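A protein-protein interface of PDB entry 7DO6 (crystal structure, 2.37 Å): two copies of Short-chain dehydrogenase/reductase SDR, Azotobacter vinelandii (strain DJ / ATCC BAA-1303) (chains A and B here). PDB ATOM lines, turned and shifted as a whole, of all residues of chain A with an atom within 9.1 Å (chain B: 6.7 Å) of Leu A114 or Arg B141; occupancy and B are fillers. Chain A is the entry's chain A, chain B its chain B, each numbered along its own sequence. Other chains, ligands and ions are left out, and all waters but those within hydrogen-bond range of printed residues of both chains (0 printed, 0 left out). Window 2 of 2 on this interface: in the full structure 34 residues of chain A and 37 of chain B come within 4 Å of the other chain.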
ATOM      1  N   HIS A 111     -15.162  12.087 -26.438  1.00  0.00           N
ATOM      2  CA  HIS A 111     -15.965  10.958 -25.988  1.00  0.00           C
ATOM      3  C   HIS A 111     -17.115  11.474 -25.134  1.00  0.00           C
ATOM      4  O   HIS A 111     -16.943  12.426 -24.369  1.00  0.00           O
ATOM      5  CB  HIS A 111     -15.116   9.962 -25.184  1.00  0.00           C
ATOM      6  CG  HIS A 111     -15.662   8.569 -25.177  1.00  0.00           C
ATOM      7  ND1 HIS A 111     -16.723   8.190 -24.383  1.00  0.00           N
ATOM      8  CD2 HIS A 111     -15.291   7.463 -25.864  1.00  0.00           C
ATOM      9  CE1 HIS A 111     -16.985   6.909 -24.584  1.00  0.00           C
ATOM     10  NE2 HIS A 111     -16.130   6.445 -25.479  1.00  0.00           N
ATOM     11  N   SER A 112     -18.277  10.838 -25.265  1.00  0.00           N
ATOM     12  CA  SER A 112     -19.437  11.235 -24.483  1.00  0.00           C
ATOM     13  C   SER A 112     -19.248  10.874 -23.009  1.00  0.00           C
ATOM     14  O   SER A 112     -18.442  10.010 -22.646  1.00  0.00           O
ATOM     15  CB  SER A 112     -20.708  10.585 -25.033  1.00  0.00           C
ATOM     16  OG  SER A 112     -20.564   9.182 -25.139  1.00  0.00           O
ATOM     17  N   PHE A 113     -20.023  11.549 -22.156  1.00  0.00           N
ATOM     18  CA  PHE A 113     -19.776  11.521 -20.717  1.00  0.00           C
ATOM     19  C   PHE A 113     -20.415  10.308 -20.045  1.00  0.00           C
ATOM     20  O   PHE A 113     -19.747   9.580 -19.301  1.00  0.00           O
ATOM     21  CB  PHE A 113     -20.288  12.820 -20.087  1.00  0.00           C
ATOM     22  CG  PHE A 113     -20.422  12.762 -18.591  1.00  0.00           C
ATOM     23  CD1 PHE A 113     -19.301  12.740 -17.781  1.00  0.00           C
ATOM     24  CD2 PHE A 113     -21.673  12.741 -17.996  1.00  0.00           C
ATOM     25  CE1 PHE A 113     -19.421  12.694 -16.403  1.00  0.00           C
ATOM     26  CE2 PHE A 113     -21.801  12.695 -16.619  1.00  0.00           C
ATOM     27  CZ  PHE A 113     -20.672  12.672 -15.822  1.00  0.00           C
ATOM     28  N   LEU A 114     -21.705  10.075 -20.297  1.00  0.00           N
ATOM     29  CA  LEU A 114     -22.452   9.066 -19.552  1.00  0.00           C
ATOM     30  C   LEU A 114     -21.949   7.647 -19.782  1.00  0.00           C
ATOM     31  O   LEU A 114     -22.351   6.742 -19.043  1.00  0.00           O
ATOM     32  CB  LEU A 114     -23.937   9.143 -19.909  1.00  0.00           C
ATOM     33  CG  LEU A 114     -24.670  10.388 -19.406  1.00  0.00           C
ATOM     34  CD1 LEU A 114     -26.110  10.406 -19.897  1.00  0.00           C
ATOM     35  CD2 LEU A 114     -24.612  10.460 -17.889  1.00  0.00           C
ATOM     36  N   ASP A 115     -21.089   7.425 -20.779  1.00  0.00           N
ATOM     37  CA  ASP A 115     -20.544   6.102 -21.056  1.00  0.00           C
ATOM     38  C   ASP A 115     -19.022   6.137 -21.111  1.00  0.00           C
ATOM     39  O   ASP A 115     -18.402   5.294 -21.763  1.00  0.00           O
ATOM     40  CB  ASP A 115     -21.111   5.537 -22.359  1.00  0.00           C
ATOM     41  CG  ASP A 115     -20.813   6.421 -23.557  1.00  0.00           C
ATOM     42  OD1 ASP A 115     -20.761   7.657 -23.386  1.00  0.00           O
ATOM     43  OD2 ASP A 115     -20.632   5.881 -24.668  1.00  0.00           O
ATOM     44  N   MET A 116     -18.412   7.100 -20.437  1.00  0.00           N
ATOM     45  CA  MET A 116     -16.959   7.216 -20.431  1.00  0.00           C
ATOM     46  C   MET A 116     -16.339   6.032 -19.700  1.00  0.00           C
ATOM     47  O   MET A 116     -16.611   5.841 -18.507  1.00  0.00           O
ATOM     48  CB  MET A 116     -16.534   8.523 -19.771  1.00  0.00           C
ATOM     49  CG  MET A 116     -15.029   8.683 -19.630  1.00  0.00           C
ATOM     50  SD  MET A 116     -14.225   9.004 -21.212  1.00  0.00           S
ATOM     51  CE  MET A 116     -14.922  10.603 -21.617  1.00  0.00           C
ATOM     52  N   PRO A 117     -15.518   5.219 -20.358  1.00  0.00           N
ATOM     53  CA  PRO A 117     -14.856   4.119 -19.652  1.00  0.00           C
ATOM     54  C   PRO A 117     -13.725   4.628 -18.773  1.00  0.00           C
ATOM     55  O   PRO A 117     -13.119   5.670 -19.041  1.00  0.00           O
ATOM     56  CB  PRO A 117     -14.327   3.234 -20.788  1.00  0.00           C
ATOM     57  CG  PRO A 117     -14.117   4.183 -21.925  1.00  0.00           C
ATOM     58  CD  PRO A 117     -15.188   5.241 -21.795  1.00  0.00           C
ATOM     59  N   ALA A 165     -18.936  19.327 -23.803  1.00  0.00           N
ATOM     60  CA  ALA A 165     -19.727  18.125 -23.543  1.00  0.00           C
ATOM     61  C   ALA A 165     -18.948  16.855 -23.868  1.00  0.00           C
ATOM     62  O   ALA A 165     -19.068  15.848 -23.160  1.00  0.00           O
ATOM     63  CB  ALA A 165     -21.026  18.167 -24.345  1.00  0.00           C
ATOM     64  N   MET A 166     -18.160  16.874 -24.938  1.00  0.00           N
ATOM     65  CA  MET A 166     -17.326  15.738 -25.299  1.00  0.00           C
ATOM     66  C   MET A 166     -15.954  15.792 -24.642  1.00  0.00           C
ATOM     67  O   MET A 166     -15.053  15.057 -25.058  1.00  0.00           O
ATOM     68  CB  MET A 166     -17.173  15.656 -26.820  1.00  0.00           C
ATOM     69  CG  MET A 166     -18.489  15.526 -27.571  1.00  0.00           C
ATOM     70  SD  MET A 166     -19.347  13.985 -27.193  1.00  0.00           S
ATOM     71  CE  MET A 166     -18.470  12.831 -28.248  1.00  0.00           C
ATOM     72  N   THR A 168     -15.589  16.113 -20.905  1.00  0.00           N
ATOM     73  CA  THR A 168     -15.745  16.078 -19.451  1.00  0.00           C
ATOM     74  C   THR A 168     -14.506  15.517 -18.767  1.00  0.00           C
ATOM     75  O   THR A 168     -14.217  15.873 -17.618  1.00  0.00           O
ATOM     76  CB  THR A 168     -16.969  15.248 -19.061  1.00  0.00           C
ATOM     77  OG1 THR A 168     -16.883  13.950 -19.664  1.00  0.00           O
ATOM     78  CG2 THR A 168     -18.252  15.937 -19.508  1.00  0.00           C
ATOM     79  N   GLU B  85     -21.641   3.655  -8.269  1.00  0.00           N
ATOM     80  CA  GLU B  85     -22.784   2.781  -8.482  1.00  0.00           C
ATOM     81  C   GLU B  85     -23.246   2.094  -7.204  1.00  0.00           C
ATOM     82  O   GLU B  85     -24.386   1.621  -7.151  1.00  0.00           O
ATOM     83  CB  GLU B  85     -22.459   1.731  -9.546  1.00  0.00           C
ATOM     84  CG  GLU B  85     -22.773   2.184 -10.963  1.00  0.00           C
ATOM     85  CD  GLU B  85     -24.237   2.549 -11.150  1.00  0.00           C
ATOM     86  OE1 GLU B  85     -25.100   1.948 -10.473  1.00  0.00           O
ATOM     87  OE2 GLU B  85     -24.525   3.442 -11.977  1.00  0.00           O
ATOM     88  N   TYR B 133     -15.485  12.066 -10.340  1.00  0.00           N
ATOM     89  CA  TYR B 133     -15.913  11.933 -11.730  1.00  0.00           C
ATOM     90  C   TYR B 133     -16.929  10.809 -11.901  1.00  0.00           C
ATOM     91  O   TYR B 133     -18.019  11.018 -12.445  1.00  0.00           O
ATOM     92  CB  TYR B 133     -14.695  11.696 -12.627  1.00  0.00           C
ATOM     93  CG  TYR B 133     -15.009  11.650 -14.107  1.00  0.00           C
ATOM     94  CD1 TYR B 133     -15.020  12.813 -14.867  1.00  0.00           C
ATOM     95  CD2 TYR B 133     -15.287  10.448 -14.744  1.00  0.00           C
ATOM     96  CE1 TYR B 133     -15.306  12.784 -16.221  1.00  0.00           C
ATOM     97  CE2 TYR B 133     -15.576  10.409 -16.101  1.00  0.00           C
ATOM     98  CZ  TYR B 133     -15.584  11.581 -16.833  1.00  0.00           C
ATOM     99  OH  TYR B 133     -15.867  11.548 -18.181  1.00  0.00           O
ATOM    100  N   VAL B 136     -20.207  11.232 -10.030  1.00  0.00           N
ATOM    101  CA  VAL B 136     -21.088  12.092 -10.816  1.00  0.00           C
ATOM    102  C   VAL B 136     -21.715  11.308 -11.961  1.00  0.00           C
ATOM    103  O   VAL B 136     -22.919  11.418 -12.221  1.00  0.00           O
ATOM    104  CB  VAL B 136     -20.314  13.322 -11.328  1.00  0.00           C
ATOM    105  CG1 VAL B 136     -21.110  14.047 -12.404  1.00  0.00           C
ATOM    106  CG2 VAL B 136     -19.984  14.260 -10.176  1.00  0.00           C
ATOM    107  N   GLN B 137     -20.913  10.495 -12.655  1.00  0.00           N
ATOM    108  CA  GLN B 137     -21.433   9.732 -13.785  1.00  0.00           C
ATOM    109  C   GLN B 137     -22.505   8.743 -13.347  1.00  0.00           C
ATOM    110  O   GLN B 137     -23.536   8.599 -14.014  1.00  0.00           O
ATOM    111  CB  GLN B 137     -20.293   9.000 -14.491  1.00  0.00           C
ATOM    112  CG  GLN B 137     -20.751   8.094 -15.627  1.00  0.00           C
ATOM    113  CD  GLN B 137     -19.692   7.095 -16.040  1.00  0.00           C
ATOM    114  OE1 GLN B 137     -19.381   6.162 -15.300  1.00  0.00           O
ATOM    115  NE2 GLN B 137     -19.126   7.289 -17.227  1.00  0.00           N
ATOM    116  N   ALA B 138     -22.284   8.052 -12.225  1.00  0.00           N
ATOM    117  CA  ALA B 138     -23.252   7.062 -11.765  1.00  0.00           C
ATOM    118  C   ALA B 138     -24.575   7.715 -11.383  1.00  0.00           C
ATOM    119  O   ALA B 138     -25.650   7.186 -11.689  1.00  0.00           O
ATOM    120  CB  ALA B 138     -22.681   6.278 -10.588  1.00  0.00           C
ATOM    121  N   ALA B 139     -24.518   8.867 -10.714  1.00  0.00           N
ATOM    122  CA  ALA B 139     -25.745   9.575 -10.371  1.00  0.00           C
ATOM    123  C   ALA B 139     -26.409  10.161 -11.612  1.00  0.00           C
ATOM    124  O   ALA B 139     -27.640  10.133 -11.736  1.00  0.00           O
ATOM    125  CB  ALA B 139     -25.448  10.671  -9.348  1.00  0.00           C
ATOM    126  N   ALA B 140     -25.613  10.681 -12.548  1.00  0.00           N
ATOM    127  CA  ALA B 140     -26.180  11.340 -13.719  1.00  0.00           C
ATOM    128  C   ALA B 140     -26.882  10.356 -14.646  1.00  0.00           C
ATOM    129  O   ALA B 140     -27.841  10.729 -15.331  1.00  0.00           O
ATOM    130  CB  ALA B 140     -25.089  12.096 -14.475  1.00  0.00           C
ATOM    131  N   ARG B 141     -26.423   9.102 -14.689  1.00  0.00           N
ATOM    132  CA  ARG B 141     -27.081   8.112 -15.536  1.00  0.00           C
ATOM    133  C   ARG B 141     -28.443   7.726 -14.974  1.00  0.00           C
ATOM    134  O   ARG B 141     -29.398   7.513 -15.732  1.00  0.00           O
ATOM    135  CB  ARG B 141     -26.191   6.879 -15.694  1.00  0.00           C
ATOM    136  N   ARG B 142     -28.555   7.630 -13.646  1.00  0.00           N
ATOM    137  CA  ARG B 142     -29.846   7.326 -13.041  1.00  0.00           C
ATOM    138  C   ARG B 142     -30.815   8.490 -13.203  1.00  0.00           C
ATOM    139  O   ARG B 142     -32.016   8.282 -13.414  1.00  0.00           O
ATOM    140  CB  ARG B 142     -29.663   6.975 -11.565  1.00  0.00           C
ATOM    141  CG  ARG B 142     -30.964   6.755 -10.817  1.00  0.00           C
ATOM    142  CD  ARG B 142     -31.760   5.597 -11.402  1.00  0.00           C
ATOM    143  NE  ARG B 142     -33.054   5.443 -10.741  1.00  0.00           N
ATOM    144  CZ  ARG B 142     -33.800   4.343 -10.791  1.00  0.00           C
ATOM    145  NH1 ARG B 142     -34.963   4.300 -10.154  1.00  0.00           N
ATOM    146  NH2 ARG B 142     -33.382   3.283 -11.469  1.00  0.00           N
ATOM    147  N   MET B 143     -30.312   9.725 -13.111  1.00  0.00           N
ATOM    148  CA  MET B 143     -31.169  10.888 -13.322  1.00  0.00           C
ATOM    149  C   MET B 143     -31.717  10.919 -14.742  1.00  0.00           C
ATOM    150  O   MET B 143     -32.874  11.294 -14.960  1.00  0.00           O
ATOM    151  CB  MET B 143     -30.399  12.174 -13.022  1.00  0.00           C
ATOM    152  CG  MET B 143     -30.218  12.459 -11.544  1.00  0.00           C
ATOM    153  SD  MET B 143     -28.916  13.663 -11.253  1.00  0.00           S
ATOM    154  CE  MET B 143     -28.586  13.399  -9.513  1.00  0.00           C
ATOM    155  N   LYS B 144     -30.897  10.533 -15.721  1.00  0.00           N
ATOM    156  CA  LYS B 144     -31.375  10.466 -17.097  1.00  0.00           C
ATOM    157  C   LYS B 144     -32.364   9.323 -17.280  1.00  0.00           C
ATOM    158  O   LYS B 144     -33.349   9.457 -18.016  1.00  0.00           O
ATOM    159  CB  LYS B 144     -30.192  10.316 -18.052  1.00  0.00           C
ATOM    160  CG  LYS B 144     -30.558  10.395 -19.526  1.00  0.00           C
ATOM    161  CD  LYS B 144     -30.187   9.110 -20.247  1.00  0.00           C
ATOM    162  CE  LYS B 144     -29.854   9.365 -21.710  1.00  0.00           C
ATOM    163  NZ  LYS B 144     -29.310   8.145 -22.376  1.00  0.00           N
ATOM    164  N   GLU B 145     -32.123   8.191 -16.613  1.00  0.00           N
ATOM    165  CA  GLU B 145     -33.008   7.040 -16.755  1.00  0.00           C
ATOM    166  C   GLU B 145     -34.391   7.333 -16.185  1.00  0.00           C
ATOM    167  O   GLU B 145     -35.401   6.864 -16.720  1.00  0.00           O
ATOM    168  CB  GLU B 145     -32.389   5.818 -16.078  1.00  0.00           C
ATOM    169  CG  GLU B 145     -32.739   4.491 -16.736  1.00  0.00           C
ATOM    170  CD  GLU B 145     -34.119   3.992 -16.349  1.00  0.00           C
ATOM    171  OE1 GLU B 145     -34.274   3.488 -15.215  1.00  0.00           O
ATOM    172  OE2 GLU B 145     -35.049   4.102 -17.177  1.00  0.00           O
ATOM    173  N   GLN B 146     -34.457   8.109 -15.101  1.00  0.00           N
ATOM    174  CA  GLN B 146     -35.753   8.525 -14.576  1.00  0.00           C
ATOM    175  C   GLN B 146     -36.411   9.553 -15.488  1.00  0.00           C
ATOM    176  O   GLN B 146     -37.638   9.559 -15.641  1.00  0.00           O
ATOM    177  CB  GLN B 146     -35.594   9.083 -13.162  1.00  0.00           C
ATOM    178  CG  GLN B 146     -35.005   8.095 -12.168  1.00  0.00           C
ATOM    179  CD  GLN B 146     -34.362   8.778 -10.979  1.00  0.00           C
ATOM    180  OE1 GLN B 146     -33.939   8.125 -10.024  1.00  0.00           O
ATOM    181  NE2 GLN B 146     -34.286  10.106 -11.031  1.00  0.00           N
ATOM    182  N   ALA B 187     -23.225  18.703 -21.184  1.00  0.00           N
ATOM    183  CA  ALA B 187     -23.550  17.328 -21.543  1.00  0.00           C
ATOM    184  C   ALA B 187     -24.827  16.824 -20.883  1.00  0.00           C
ATOM    185  O   ALA B 187     -25.442  15.884 -21.397  1.00  0.00           O
ATOM    186  CB  ALA B 187     -22.386  16.405 -21.186  1.00  0.00           C
ATOM    187  N   LEU B 188     -25.245  17.418 -19.763  1.00  0.00           N
ATOM    188  CA  LEU B 188     -26.442  16.976 -19.059  1.00  0.00           C
ATOM    189  C   LEU B 188     -27.573  17.993 -19.082  1.00  0.00           C
ATOM    190  O   LEU B 188     -28.671  17.680 -18.608  1.00  0.00           O
ATOM    191  CB  LEU B 188     -26.107  16.631 -17.602  1.00  0.00           C
ATOM    192  CG  LEU B 188     -24.962  15.640 -17.409  1.00  0.00           C
ATOM    193  CD1 LEU B 188     -24.808  15.303 -15.939  1.00  0.00           C
ATOM    194  CD2 LEU B 188     -25.190  14.388 -18.244  1.00  0.00           C
ATOM    195  N   TYR B 191     -31.021  16.967 -20.385  1.00  0.00           N
ATOM    196  CA  TYR B 191     -31.779  16.038 -19.559  1.00  0.00           C
ATOM    197  C   TYR B 191     -32.330  16.689 -18.299  1.00  0.00           C
ATOM    198  O   TYR B 191     -32.803  15.982 -17.405  1.00  0.00           O
ATOM    199  CB  TYR B 191     -30.913  14.832 -19.188  1.00  0.00           C
ATOM    200  CG  TYR B 191     -30.253  14.170 -20.374  1.00  0.00           C
ATOM    201  CD1 TYR B 191     -31.013  13.612 -21.397  1.00  0.00           C
ATOM    202  CD2 TYR B 191     -28.871  14.105 -20.475  1.00  0.00           C
ATOM    203  CE1 TYR B 191     -30.412  13.005 -22.485  1.00  0.00           C
ATOM    204  CE2 TYR B 191     -28.260  13.500 -21.559  1.00  0.00           C
ATOM    205  CZ  TYR B 191     -29.034  12.952 -22.559  1.00  0.00           C
ATOM    206  OH  TYR B 191     -28.425  12.351 -23.635  1.00  0.00           O
ATOM    207  N   ILE B 193     -30.584  18.224 -16.007  1.00  0.00           N
ATOM    208  CA  ILE B 193     -29.635  18.022 -14.919  1.00  0.00           C
ATOM    209  C   ILE B 193     -28.776  19.273 -14.804  1.00  0.00           C
ATOM    210  O   ILE B 193     -28.032  19.613 -15.732  1.00  0.00           O
ATOM    211  CB  ILE B 193     -28.764  16.779 -15.145  1.00  0.00           C
ATOM    212  CG1 ILE B 193     -29.624  15.514 -15.135  1.00  0.00           C
ATOM    213  CG2 ILE B 193     -27.673  16.706 -14.093  1.00  0.00           C
ATOM    214  CD1 ILE B 193     -28.936  14.307 -15.743  1.00  0.00           C
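No position is printed for both chains.
Of the 13 pairs that touch across the chains among the printed residues, none has its exchanged pair printed and touching as well.
The backbone carbonyl oxygen of Phe A113 lies within hydrogen-bond range of the side-chain amide nitrogen of Gln B137.
NE2 of Gln B137 sits at hydrogen-bond distance from O of Met A116 (3.2 Å).
The side-chain hydroxyl (OG1) of Thr A168 sits at hydrogen-bond distance from the side-chain hydroxyl (OH) of Tyr B133, 3.0 Å away.
His A111 touches none of the printed residues of chain B.
Of the printed residues of chain B, Leu A114 touches Gln B137 (3.7 Å), Ala B140 (3.8 Å), Arg B141 (3.9 Å) and Leu B188 (3.99 Å).
Printed residues of chain B within 4 Å of Thr A168: Tyr B133 (3.0 Å).
Of the printed residues of chain A, Val B136 touches Phe A113.
Of the printed residues of chain A, Arg B141 touches Leu A114 (3.9 Å).
No residue of chain A comes within 4 Å of Lys B144.
The nearest printed residue of chain B that does not touch Leu A114 is Tyr B191 (4.1 Å).
The nearest residue of chain A that does not touch Arg B141 is Phe A113 (6.2 Å).
The nearest printed residue of chain A that does not touch Val B136 is Leu A114 (6.0 Å).
The backbone NH of Ile B193 lies within hydrogen-bond range of the backbone carbonyl oxygen of Leu B188 (3.3 Å).
Among the printed residues, merely in contact across the chains: Phe A113 with Tyr B133 (3.7 Å), Phe A113 with Val B136 (3.7 Å), Phe A113 with Ala B140 (3.97 Å), Phe A113 with Leu B188 (3.9 Å), Leu A114 with Gln B137 (3.7 Å), Leu A114 with Ala B140 (3.8 Å), Leu A114 with Arg B141 (3.9 Å), Leu A114 with Leu B188 (3.99 Å), Met A116 with Tyr B133 (3.3 Å) and Ala A165 with Ala B187 (3.9 Å).
Of the 10 printed residues of chain A, 5 touch a printed residue of chain B.
Hydrophobic or aromatic side chains of chain A that line the printed part of chain B: Phe A113, Leu A114, Met A116 and Ala A165.
Of the 17 printed residues of chain B, 7 touch a printed residue of chain A.
Hydrophobic or aromatic side chains of chain B within 4 Å of the printed part of chain A: Tyr B133, Val B136, Ala B140, Ala B187 and Leu B188.
Among the printed residues, no Asp or Glu carboxylate lies within 4 Å of a Lys or Arg side-chain nitrogen of the other chain.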
